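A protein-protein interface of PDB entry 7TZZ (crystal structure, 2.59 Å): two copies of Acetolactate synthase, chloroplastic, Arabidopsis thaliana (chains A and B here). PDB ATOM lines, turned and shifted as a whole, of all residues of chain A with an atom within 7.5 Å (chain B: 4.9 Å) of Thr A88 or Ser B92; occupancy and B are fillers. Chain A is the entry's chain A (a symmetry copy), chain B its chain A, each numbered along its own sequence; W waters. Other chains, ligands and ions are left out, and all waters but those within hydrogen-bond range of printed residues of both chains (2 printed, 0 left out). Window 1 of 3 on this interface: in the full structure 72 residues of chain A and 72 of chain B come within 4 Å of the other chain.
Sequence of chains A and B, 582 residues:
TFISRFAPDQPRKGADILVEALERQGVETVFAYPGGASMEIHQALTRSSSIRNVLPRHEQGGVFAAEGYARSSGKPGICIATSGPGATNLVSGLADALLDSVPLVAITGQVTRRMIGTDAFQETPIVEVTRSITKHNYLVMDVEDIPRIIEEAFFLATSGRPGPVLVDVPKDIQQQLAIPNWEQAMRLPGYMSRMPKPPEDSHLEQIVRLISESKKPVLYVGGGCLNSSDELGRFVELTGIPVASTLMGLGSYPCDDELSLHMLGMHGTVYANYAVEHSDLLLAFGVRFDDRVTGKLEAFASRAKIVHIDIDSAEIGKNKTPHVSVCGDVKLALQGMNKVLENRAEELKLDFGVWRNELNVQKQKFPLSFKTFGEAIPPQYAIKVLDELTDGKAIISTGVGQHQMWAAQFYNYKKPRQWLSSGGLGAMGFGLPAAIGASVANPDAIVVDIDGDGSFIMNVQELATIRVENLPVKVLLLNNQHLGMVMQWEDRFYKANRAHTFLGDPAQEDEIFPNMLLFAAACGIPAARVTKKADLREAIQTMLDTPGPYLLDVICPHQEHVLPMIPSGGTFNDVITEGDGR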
ATOM      1  N   HIS A  58      33.427 -20.767  28.907  1.00  0.00           N
ATOM      2  CA  HIS A  58      32.421 -20.441  27.911  1.00  0.00           C
ATOM      3  C   HIS A  58      32.147 -21.723  27.136  1.00  0.00           C
ATOM      4  O   HIS A  58      33.093 -22.452  26.811  1.00  0.00           O
ATOM      5  CB  HIS A  58      32.935 -19.338  26.997  1.00  0.00           C
ATOM      6  CG  HIS A  58      31.896 -18.716  26.116  1.00  0.00           C
ATOM      7  ND1 HIS A  58      31.244 -19.410  25.117  1.00  0.00           N
ATOM      8  CD2 HIS A  58      31.465 -17.434  26.022  1.00  0.00           C
ATOM      9  CE1 HIS A  58      30.428 -18.590  24.477  1.00  0.00           C
ATOM     10  NE2 HIS A  58      30.547 -17.383  25.002  1.00  0.00           N
ATOM     11  N   GLU A  59      30.865 -22.011  26.849  1.00  0.00           N
ATOM     12  CA  GLU A  59      30.556 -23.258  26.142  1.00  0.00           C
ATOM     13  C   GLU A  59      31.243 -23.318  24.778  1.00  0.00           C
ATOM     14  O   GLU A  59      31.568 -24.414  24.296  1.00  0.00           O
ATOM     15  CB  GLU A  59      29.044 -23.441  25.988  1.00  0.00           C
ATOM     16  CG  GLU A  59      28.343 -23.606  27.315  1.00  0.00           C
ATOM     17  CD  GLU A  59      27.895 -22.266  27.878  1.00  0.00           C
ATOM     18  OE1 GLU A  59      28.353 -21.217  27.350  1.00  0.00           O
ATOM     19  OE2 GLU A  59      27.077 -22.245  28.831  1.00  0.00           O
ATOM     20  N   GLN A  60      31.502 -22.165  24.143  1.00  0.00           N
ATOM     21  CA  GLN A  60      32.285 -22.222  22.919  1.00  0.00           C
ATOM     22  C   GLN A  60      33.681 -22.752  23.215  1.00  0.00           C
ATOM     23  O   GLN A  60      34.235 -23.546  22.442  1.00  0.00           O
ATOM     24  CB  GLN A  60      32.350 -20.859  22.242  1.00  0.00           C
ATOM     25  CG  GLN A  60      33.125 -20.980  20.941  1.00  0.00           C
ATOM     26  CD  GLN A  60      33.065 -19.743  20.064  1.00  0.00           C
ATOM     27  OE1 GLN A  60      34.017 -18.972  20.006  1.00  0.00           O
ATOM     28  NE2 GLN A  60      31.969 -19.589  19.317  1.00  0.00           N
ATOM     29  N   ALA A  81      26.263 -29.125  27.738  1.00  0.00           N
ATOM     30  CA  ALA A  81      25.854 -27.749  27.983  1.00  0.00           C
ATOM     31  C   ALA A  81      24.421 -27.722  28.484  1.00  0.00           C
ATOM     32  O   ALA A  81      23.629 -28.644  28.250  1.00  0.00           O
ATOM     33  CB  ALA A  81      26.030 -26.886  26.722  1.00  0.00           C
ATOM     34  N   THR A  82      24.084 -26.649  29.178  1.00  0.00           N
ATOM     35  CA  THR A  82      22.701 -26.498  29.585  1.00  0.00           C
ATOM     36  C   THR A  82      21.816 -26.107  28.390  1.00  0.00           C
ATOM     37  O   THR A  82      22.267 -25.974  27.254  1.00  0.00           O
ATOM     38  CB  THR A  82      22.596 -25.510  30.752  1.00  0.00           C
ATOM     39  OG1 THR A  82      21.309 -25.674  31.361  1.00  0.00           O
ATOM     40  CG2 THR A  82      22.741 -24.050  30.306  1.00  0.00           C
ATOM     41  N   SER A  83      20.522 -25.930  28.650  1.00  0.00           N
ATOM     42  CA  SER A  83      19.590 -25.545  27.604  1.00  0.00           C
ATOM     43  C   SER A  83      19.850 -24.104  27.155  1.00  0.00           C
ATOM     44  O   SER A  83      20.740 -23.420  27.659  1.00  0.00           O
ATOM     45  CB  SER A  83      18.156 -25.722  28.097  1.00  0.00           C
ATOM     46  OG  SER A  83      17.843 -24.808  29.138  1.00  0.00           O
ATOM     47  N   GLY A  84      19.065 -23.650  26.168  1.00  0.00           N
ATOM     48  CA  GLY A  84      19.030 -22.255  25.790  1.00  0.00           C
ATOM     49  C   GLY A  84      20.375 -21.698  25.380  1.00  0.00           C
ATOM     50  O   GLY A  84      20.989 -22.120  24.389  1.00  0.00           O
ATOM     51  N   PRO A  85      20.869 -20.738  26.155  1.00  0.00           N
ATOM     52  CA  PRO A  85      22.149 -20.092  25.799  1.00  0.00           C
ATOM     53  C   PRO A  85      23.339 -21.031  25.908  1.00  0.00           C
ATOM     54  O   PRO A  85      24.368 -20.826  25.234  1.00  0.00           O
ATOM     55  CB  PRO A  85      22.237 -18.922  26.803  1.00  0.00           C
ATOM     56  CG  PRO A  85      21.509 -19.435  28.028  1.00  0.00           C
ATOM     57  CD  PRO A  85      20.386 -20.352  27.498  1.00  0.00           C
ATOM     58  N   GLY A  86      23.240 -22.061  26.753  1.00  0.00           N
ATOM     59  CA  GLY A  86      24.269 -23.072  26.741  1.00  0.00           C
ATOM     60  C   GLY A  86      24.348 -23.732  25.383  1.00  0.00           C
ATOM     61  O   GLY A  86      25.406 -23.774  24.754  1.00  0.00           O
ATOM     62  N   ALA A  87      23.201 -24.192  24.886  1.00  0.00           N
ATOM     63  CA  ALA A  87      23.153 -24.902  23.621  1.00  0.00           C
ATOM     64  C   ALA A  87      23.557 -23.989  22.470  1.00  0.00           C
ATOM     65  O   ALA A  87      24.363 -24.380  21.617  1.00  0.00           O
ATOM     66  CB  ALA A  87      21.753 -25.495  23.408  1.00  0.00           C
ATOM     67  N   THR A  88      23.020 -22.758  22.423  1.00  0.00           N
ATOM     68  CA  THR A  88      23.373 -21.914  21.282  1.00  0.00           C
ATOM     69  C   THR A  88      24.861 -21.576  21.278  1.00  0.00           C
ATOM     70  O   THR A  88      25.435 -21.363  20.206  1.00  0.00           O
ATOM     71  CB  THR A  88      22.536 -20.626  21.229  1.00  0.00           C
ATOM     72  OG1 THR A  88      22.683 -19.886  22.444  1.00  0.00           O
ATOM     73  CG2 THR A  88      21.088 -20.909  20.982  1.00  0.00           C
ATOM     74  N   ASN A  89      25.513 -21.553  22.444  1.00  0.00           N
ATOM     75  CA  ASN A  89      26.955 -21.302  22.461  1.00  0.00           C
ATOM     76  C   ASN A  89      27.786 -22.451  21.897  1.00  0.00           C
ATOM     77  O   ASN A  89      28.991 -22.264  21.686  1.00  0.00           O
ATOM     78  CB  ASN A  89      27.441 -21.011  23.880  1.00  0.00           C
ATOM     79  CG  ASN A  89      27.171 -19.580  24.307  1.00  0.00           C
ATOM     80  OD1 ASN A  89      26.889 -18.735  23.468  1.00  0.00           O
ATOM     81  ND2 ASN A  89      27.262 -19.301  25.622  1.00  0.00           N
ATOM     82  N   LEU A  90      27.198 -23.635  21.661  1.00  0.00           N
ATOM     83  CA  LEU A  90      27.943 -24.733  21.041  1.00  0.00           C
ATOM     84  C   LEU A  90      27.995 -24.627  19.532  1.00  0.00           C
ATOM     85  O   LEU A  90      28.779 -25.349  18.912  1.00  0.00           O
ATOM     86  CB  LEU A  90      27.313 -26.087  21.351  1.00  0.00           C
ATOM     87  CG  LEU A  90      27.118 -26.455  22.800  1.00  0.00           C
ATOM     88  CD1 LEU A  90      26.415 -27.769  22.812  1.00  0.00           C
ATOM     89  CD2 LEU A  90      28.467 -26.548  23.474  1.00  0.00           C
ATOM     90  N   VAL A  91      27.168 -23.771  18.934  1.00  0.00           N
ATOM     91  CA  VAL A  91      26.819 -23.911  17.520  1.00  0.00           C
ATOM     92  C   VAL A  91      28.047 -23.784  16.600  1.00  0.00           C
ATOM     93  O   VAL A  91      28.217 -24.577  15.661  1.00  0.00           O
ATOM     94  CB  VAL A  91      25.709 -22.905  17.177  1.00  0.00           C
ATOM     95  CG1 VAL A  91      25.751 -22.529  15.710  1.00  0.00           C
ATOM     96  CG2 VAL A  91      24.331 -23.488  17.633  1.00  0.00           C
ATOM     97  N   SER A  92      28.941 -22.830  16.858  1.00  0.00           N
ATOM     98  CA  SER A  92      30.123 -22.708  16.007  1.00  0.00           C
ATOM     99  C   SER A  92      30.980 -23.968  16.052  1.00  0.00           C
ATOM    100  O   SER A  92      31.564 -24.348  15.035  1.00  0.00           O
ATOM    101  CB  SER A  92      30.958 -21.487  16.399  1.00  0.00           C
ATOM    102  OG  SER A  92      30.229 -20.293  16.190  1.00  0.00           O
ATOM    103  N   GLY A  93      31.030 -24.658  17.197  1.00  0.00           N
ATOM    104  CA  GLY A  93      31.843 -25.864  17.283  1.00  0.00           C
ATOM    105  C   GLY A  93      31.230 -27.035  16.545  1.00  0.00           C
ATOM    106  O   GLY A  93      31.942 -27.821  15.896  1.00  0.00           O
ATOM    107  N   LEU A  94      29.906 -27.170  16.631  1.00  0.00           N
ATOM    108  CA  LEU A  94      29.190 -28.163  15.831  1.00  0.00           C
ATOM    109  C   LEU A  94      29.452 -27.961  14.336  1.00  0.00           C
ATOM    110  O   LEU A  94      29.831 -28.908  13.623  1.00  0.00           O
ATOM    111  CB  LEU A  94      27.688 -28.070  16.124  1.00  0.00           C
ATOM    112  CG  LEU A  94      27.323 -28.204  17.594  1.00  0.00           C
ATOM    113  CD1 LEU A  94      25.837 -28.162  17.811  1.00  0.00           C
ATOM    114  CD2 LEU A  94      27.887 -29.509  18.123  1.00  0.00           C
ATOM    115  N   THR A 108      23.013 -31.695  25.352  1.00  0.00           N
ATOM    116  CA  THR A 108      22.406 -30.469  25.873  1.00  0.00           C
ATOM    117  C   THR A 108      21.227 -30.802  26.785  1.00  0.00           C
ATOM    118  O   THR A 108      20.370 -31.646  26.471  1.00  0.00           O
ATOM    119  CB  THR A 108      21.958 -29.495  24.732  1.00  0.00           C
ATOM    120  OG1 THR A 108      21.126 -30.185  23.791  1.00  0.00           O
ATOM    121  CG2 THR A 108      23.143 -28.874  23.990  1.00  0.00           C
ATOM    122  N   GLU A 123      14.666 -21.928  26.811  1.00  0.00           N
ATOM    123  CA  GLU A 123      14.318 -22.891  25.770  1.00  0.00           C
ATOM    124  C   GLU A 123      14.844 -22.454  24.409  1.00  0.00           C
ATOM    125  O   GLU A 123      14.627 -21.315  23.972  1.00  0.00           O
ATOM    126  CB  GLU A 123      12.816 -23.116  25.658  1.00  0.00           C
ATOM    127  CG  GLU A 123      12.521 -24.246  24.670  1.00  0.00           C
ATOM    128  CD  GLU A 123      11.043 -24.333  24.260  1.00  0.00           C
ATOM    129  OE1 GLU A 123      10.207 -23.608  24.872  1.00  0.00           O
ATOM    130  OE2 GLU A 123      10.719 -25.145  23.353  1.00  0.00           O
ATOM    131  N   THR A 124      15.516 -23.372  23.736  1.00  0.00           N
ATOM    132  CA  THR A 124      15.930 -23.166  22.373  1.00  0.00           C
ATOM    133  C   THR A 124      15.541 -24.433  21.633  1.00  0.00           C
ATOM    134  O   THR A 124      15.770 -25.545  22.145  1.00  0.00           O
ATOM    135  CB  THR A 124      17.449 -22.901  22.253  1.00  0.00           C
ATOM    136  OG1 THR A 124      17.714 -21.606  22.768  1.00  0.00           O
ATOM    137  CG2 THR A 124      17.871 -22.892  20.829  1.00  0.00           C
ATOM    138  N   PRO A 125      14.962 -24.315  20.461  1.00  0.00           N
ATOM    139  CA  PRO A 125      14.716 -25.508  19.641  1.00  0.00           C
ATOM    140  C   PRO A 125      16.018 -26.020  19.020  1.00  0.00           C
ATOM    141  O   PRO A 125      16.221 -25.940  17.796  1.00  0.00           O
ATOM    142  CB  PRO A 125      13.698 -24.998  18.594  1.00  0.00           C
ATOM    143  CG  PRO A 125      14.002 -23.562  18.407  1.00  0.00           C
ATOM    144  CD  PRO A 125      14.501 -23.069  19.814  1.00  0.00           C
ATOM    145  N   ILE A 126      16.911 -26.562  19.858  1.00  0.00           N
ATOM    146  CA  ILE A 126      18.299 -26.768  19.427  1.00  0.00           C
ATOM    147  C   ILE A 126      18.382 -27.874  18.378  1.00  0.00           C
ATOM    148  O   ILE A 126      19.306 -27.884  17.546  1.00  0.00           O
ATOM    149  CB  ILE A 126      19.228 -27.056  20.636  1.00  0.00           C
ATOM    150  CG1 ILE A 126      20.710 -26.962  20.225  1.00  0.00           C
ATOM    151  CG2 ILE A 126      18.973 -28.432  21.233  1.00  0.00           C
ATOM    152  CD1 ILE A 126      21.121 -25.547  19.819  1.00  0.00           C
ATOM    153  N   VAL A 129      17.673 -26.029  15.190  1.00  0.00           N
ATOM    154  CA  VAL A 129      18.783 -25.135  14.898  1.00  0.00           C
ATOM    155  C   VAL A 129      19.948 -25.908  14.308  1.00  0.00           C
ATOM    156  O   VAL A 129      20.575 -25.456  13.344  1.00  0.00           O
ATOM    157  CB  VAL A 129      19.193 -24.385  16.182  1.00  0.00           C
ATOM    158  CG1 VAL A 129      20.546 -23.685  15.994  1.00  0.00           C
ATOM    159  CG2 VAL A 129      18.130 -23.401  16.579  1.00  0.00           C
ATOM    160  N   THR A 130      20.251 -27.094  14.864  1.00  0.00           N
ATOM    161  CA  THR A 130      21.491 -27.784  14.543  1.00  0.00           C
ATOM    162  C   THR A 130      21.330 -28.897  13.522  1.00  0.00           C
ATOM    163  O   THR A 130      22.337 -29.533  13.156  1.00  0.00           O
ATOM    164  CB  THR A 130      22.160 -28.339  15.817  1.00  0.00           C
ATOM    165  OG1 THR A 130      21.314 -29.308  16.452  1.00  0.00           O
ATOM    166  CG2 THR A 130      22.466 -27.215  16.779  1.00  0.00           C
ATOM    167  N   GLN B  60      29.689 -12.437  19.062  1.00  0.00           N
ATOM    168  CA  GLN B  60      28.716 -12.491  20.141  1.00  0.00           C
ATOM    169  C   GLN B  60      28.686 -11.163  20.886  1.00  0.00           C
ATOM    170  O   GLN B  60      27.614 -10.672  21.264  1.00  0.00           O
ATOM    171  CB  GLN B  60      29.011 -13.644  21.094  1.00  0.00           C
ATOM    172  CG  GLN B  60      27.938 -13.698  22.166  1.00  0.00           C
ATOM    173  CD  GLN B  60      27.992 -14.938  23.039  1.00  0.00           C
ATOM    174  OE1 GLN B  60      28.454 -14.883  24.174  1.00  0.00           O
ATOM    175  NE2 GLN B  60      27.449 -16.050  22.538  1.00  0.00           N
ATOM    176  N   PHE B  64      25.306  -8.842  21.113  1.00  0.00           N
ATOM    177  CA  PHE B  64      24.818  -8.400  22.426  1.00  0.00           C
ATOM    178  C   PHE B  64      24.896  -6.868  22.554  1.00  0.00           C
ATOM    179  O   PHE B  64      24.015  -6.256  23.159  1.00  0.00           O
ATOM    180  CB  PHE B  64      25.591  -9.081  23.565  1.00  0.00           C
ATOM    181  CG  PHE B  64      25.206 -10.531  23.822  1.00  0.00           C
ATOM    182  CD1 PHE B  64      23.988 -11.045  23.394  1.00  0.00           C
ATOM    183  CD2 PHE B  64      26.074 -11.377  24.515  1.00  0.00           C
ATOM    184  CE1 PHE B  64      23.640 -12.390  23.645  1.00  0.00           C
ATOM    185  CE2 PHE B  64      25.743 -12.723  24.780  1.00  0.00           C
ATOM    186  CZ  PHE B  64      24.528 -13.240  24.348  1.00  0.00           C
ATOM    187  N   ASN B  89      28.469 -17.260  15.271  1.00  0.00           N
ATOM    188  CA  ASN B  89      28.695 -16.537  16.524  1.00  0.00           C
ATOM    189  C   ASN B  89      27.582 -15.552  16.874  1.00  0.00           C
ATOM    190  O   ASN B  89      27.578 -15.038  17.999  1.00  0.00           O
ATOM    191  CB  ASN B  89      30.016 -15.772  16.482  1.00  0.00           C
ATOM    192  CG  ASN B  89      31.214 -16.662  16.761  1.00  0.00           C
ATOM    193  OD1 ASN B  89      31.051 -17.767  17.262  1.00  0.00           O
ATOM    194  ND2 ASN B  89      32.430 -16.177  16.441  1.00  0.00           N
ATOM    195  N   LEU B  90      26.651 -15.256  15.952  1.00  0.00           N
ATOM    196  CA  LEU B  90      25.522 -14.381  16.280  1.00  0.00           C
ATOM    197  C   LEU B  90      24.393 -15.117  16.968  1.00  0.00           C
ATOM    198  O   LEU B  90      23.495 -14.462  17.502  1.00  0.00           O
ATOM    199  CB  LEU B  90      24.919 -13.748  15.031  1.00  0.00           C
ATOM    200  CG  LEU B  90      25.837 -12.958  14.132  1.00  0.00           C
ATOM    201  CD1 LEU B  90      25.019 -12.532  12.962  1.00  0.00           C
ATOM    202  CD2 LEU B  90      26.369 -11.766  14.891  1.00  0.00           C
ATOM    203  N   VAL B  91      24.405 -16.449  16.946  1.00  0.00           N
ATOM    204  CA  VAL B  91      23.185 -17.225  17.165  1.00  0.00           C
ATOM    205  C   VAL B  91      22.582 -16.987  18.562  1.00  0.00           C
ATOM    206  O   VAL B  91      21.363 -16.807  18.701  1.00  0.00           O
ATOM    207  CB  VAL B  91      23.478 -18.709  16.886  1.00  0.00           C
ATOM    208  CG1 VAL B  91      22.546 -19.605  17.675  1.00  0.00           C
ATOM    209  CG2 VAL B  91      23.429 -18.959  15.344  1.00  0.00           C
ATOM    210  N   SER B  92      23.404 -16.939  19.610  1.00  0.00           N
ATOM    211  CA  SER B  92      22.853 -16.693  20.941  1.00  0.00           C
ATOM    212  C   SER B  92      22.158 -15.339  21.019  1.00  0.00           C
ATOM    213  O   SER B  92      21.144 -15.210  21.710  1.00  0.00           O
ATOM    214  CB  SER B  92      23.939 -16.791  22.014  1.00  0.00           C
ATOM    215  OG  SER B  92      24.470 -18.101  22.070  1.00  0.00           O
ATOM    216  N   GLY B  93      22.646 -14.334  20.286  1.00  0.00           N
ATOM    217  CA  GLY B  93      22.015 -13.021  20.337  1.00  0.00           C
ATOM    218  C   GLY B  93      20.693 -12.981  19.602  1.00  0.00           C
ATOM    219  O   GLY B  93      19.729 -12.342  20.060  1.00  0.00           O
ATOM    220  N   LEU B  94      20.625 -13.659  18.455  1.00  0.00           N
ATOM    221  CA  LEU B  94      19.357 -13.824  17.745  1.00  0.00           C
ATOM    222  C   LEU B  94      18.306 -14.487  18.638  1.00  0.00           C
ATOM    223  O   LEU B  94      17.180 -13.977  18.783  1.00  0.00           O
ATOM    224  CB  LEU B  94      19.585 -14.661  16.481  1.00  0.00           C
ATOM    225  CG  LEU B  94      20.654 -14.116  15.547  1.00  0.00           C
ATOM    226  CD1 LEU B  94      20.790 -14.947  14.303  1.00  0.00           C
ATOM    227  CD2 LEU B  94      20.303 -12.687  15.181  1.00  0.00           C
ATOM    228  N   ALA B  95      18.637 -15.656  19.212  1.00  0.00           N
ATOM    229  CA  ALA B  95      17.667 -16.341  20.068  1.00  0.00           C
ATOM    230  C   ALA B  95      17.274 -15.453  21.236  1.00  0.00           C
ATOM    231  O   ALA B  95      16.111 -15.433  21.660  1.00  0.00           O
ATOM    232  CB  ALA B  95      18.239 -17.658  20.589  1.00  0.00           C
ATOM    233  N   ASP B  96      18.245 -14.708  21.772  1.00  0.00           N
ATOM    234  CA  ASP B  96      17.986 -13.809  22.888  1.00  0.00           C
ATOM    235  C   ASP B  96      17.041 -12.686  22.477  1.00  0.00           C
ATOM    236  O   ASP B  96      16.044 -12.423  23.161  1.00  0.00           O
ATOM    237  CB  ASP B  96      19.312 -13.262  23.404  1.00  0.00           C
ATOM    238  CG  ASP B  96      19.182 -12.531  24.738  1.00  0.00           C
ATOM    239  OD1 ASP B  96      18.460 -12.998  25.667  1.00  0.00           O
ATOM    240  OD2 ASP B  96      19.827 -11.457  24.833  1.00  0.00           O
ATOM    241  N   LEU B 425      15.866 -16.049  27.440  1.00  0.00           N
ATOM    242  CA  LEU B 425      16.959 -16.991  27.222  1.00  0.00           C
ATOM    243  C   LEU B 425      17.931 -16.991  28.395  1.00  0.00           C
ATOM    244  O   LEU B 425      18.537 -18.028  28.692  1.00  0.00           O
ATOM    245  CB  LEU B 425      17.689 -16.663  25.920  1.00  0.00           C
ATOM    246  CG  LEU B 425      18.691 -17.670  25.393  1.00  0.00           C
ATOM    247  CD1 LEU B 425      18.006 -18.934  24.823  1.00  0.00           C
ATOM    248  CD2 LEU B 425      19.602 -16.969  24.355  1.00  0.00           C
HETATM  249  O   HOH W   1      34.700 -18.104  17.282  1.00  0.00           O
HETATM  250  O   HOH W   2      26.850 -16.288  26.196  1.00  0.00           O
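Gln A60 touches Asn B89, and with the chains exchanged Asn A89 touches Gln B60. Asn A89 touches Ser B92, and with the chains exchanged Ser A92 touches Asn B89. Positions printed for both chains: 60, 89, 90, 91, 92, 93 and 94. Of the 10 pairs that touch across the chains among the printed residues, 4 have their exchanged pair printed and touching as well.
A ring nitrogen (ND1) of His A58 sits at hydrogen-bond distance from the backbone NH (N) of Gln A60, 2.9 Å away. ND2 of Asn A89 is in hydrogen-bond range of OE1 of Glu A59 (2.8 Å). The backbone carbonyl oxygen (O) of Gly A84 sits at hydrogen-bond distance from the side-chain hydroxyl (OG1) of Thr A88 (3.4 Å). The backbone carbonyl oxygen of Pro A85 lies within hydrogen-bond range of the side-chain hydroxyl of Thr A88 (3.4 Å). The side-chain amide nitrogen (ND2) of Asn A89 sits close to the backbone carbonyl oxygen (O) of Pro A85.
Printed residues of chain B within 4 Å of Thr A88: Val B91 (3.7 Å) and Ser B92 (2.6 Å). Of the printed residues of chain B, Asn A89 touches Gln B60 and Ser B92. Of the printed residues of chain A, Val B91 touches Thr A88 (3.7 Å). Of chain A, only Thr A88 and Asn A89 come within 4 Å of Ser B92. The nearest residue of chain A that does not touch Ser B92 is Pro A85 (4.2 Å).
Water W2 bridges the side-chain amide oxygen (OE1) of Gln B60 (2.9 Å) and the side-chain amide nitrogen (ND2) of Asn A89 (3.1 Å). Water W1 bridges the side-chain amide oxygen (OE1) of Gln A60 and the side-chain amide nitrogen (ND2) of Asn B89.
Gly A84 touches Leu B425. Pro A85 touches Leu B425. Thr A88 touches Val B91 (CB to CG1, 3.7 Å). Leu B425 touches Thr A124 (CD1 to OG1, 3.4 Å).
A ring nitrogen (NE2) of His A58 lies within hydrogen-bond range of the side-chain amide oxygen (OE1) of Gln B60. The side-chain amide nitrogen (NE2) of Gln B60 lies within hydrogen-bond range of the side-chain amide oxygen (OD1) of Asn A89, 2.9 Å away. The side-chain amide nitrogen of Gln A60 is in hydrogen-bond range of the side-chain amide oxygen of Asn B89 (2.9 Å). The side-chain amide oxygen of Asn B89 is in hydrogen-bond range of the side-chain hydroxyl of Ser A92 (2.9 Å). The side-chain hydroxyl of Ser B92 is in hydrogen-bond range of the side-chain hydroxyl of Thr A88 (2.6 Å). OG of Ser B92 sits at hydrogen-bond distance from OD1 of Asn A89 (2.9 Å).
Of the 24 printed residues of chain A, 8 touch a printed residue of chain B. Hydrophobic or aromatic side chains of chain A within 4 Å of the printed part of chain B: His A58 and Pro A85. Hydrophobic or aromatic side chains of chain B that line the printed part of chain A: Val B91 and Leu B425.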
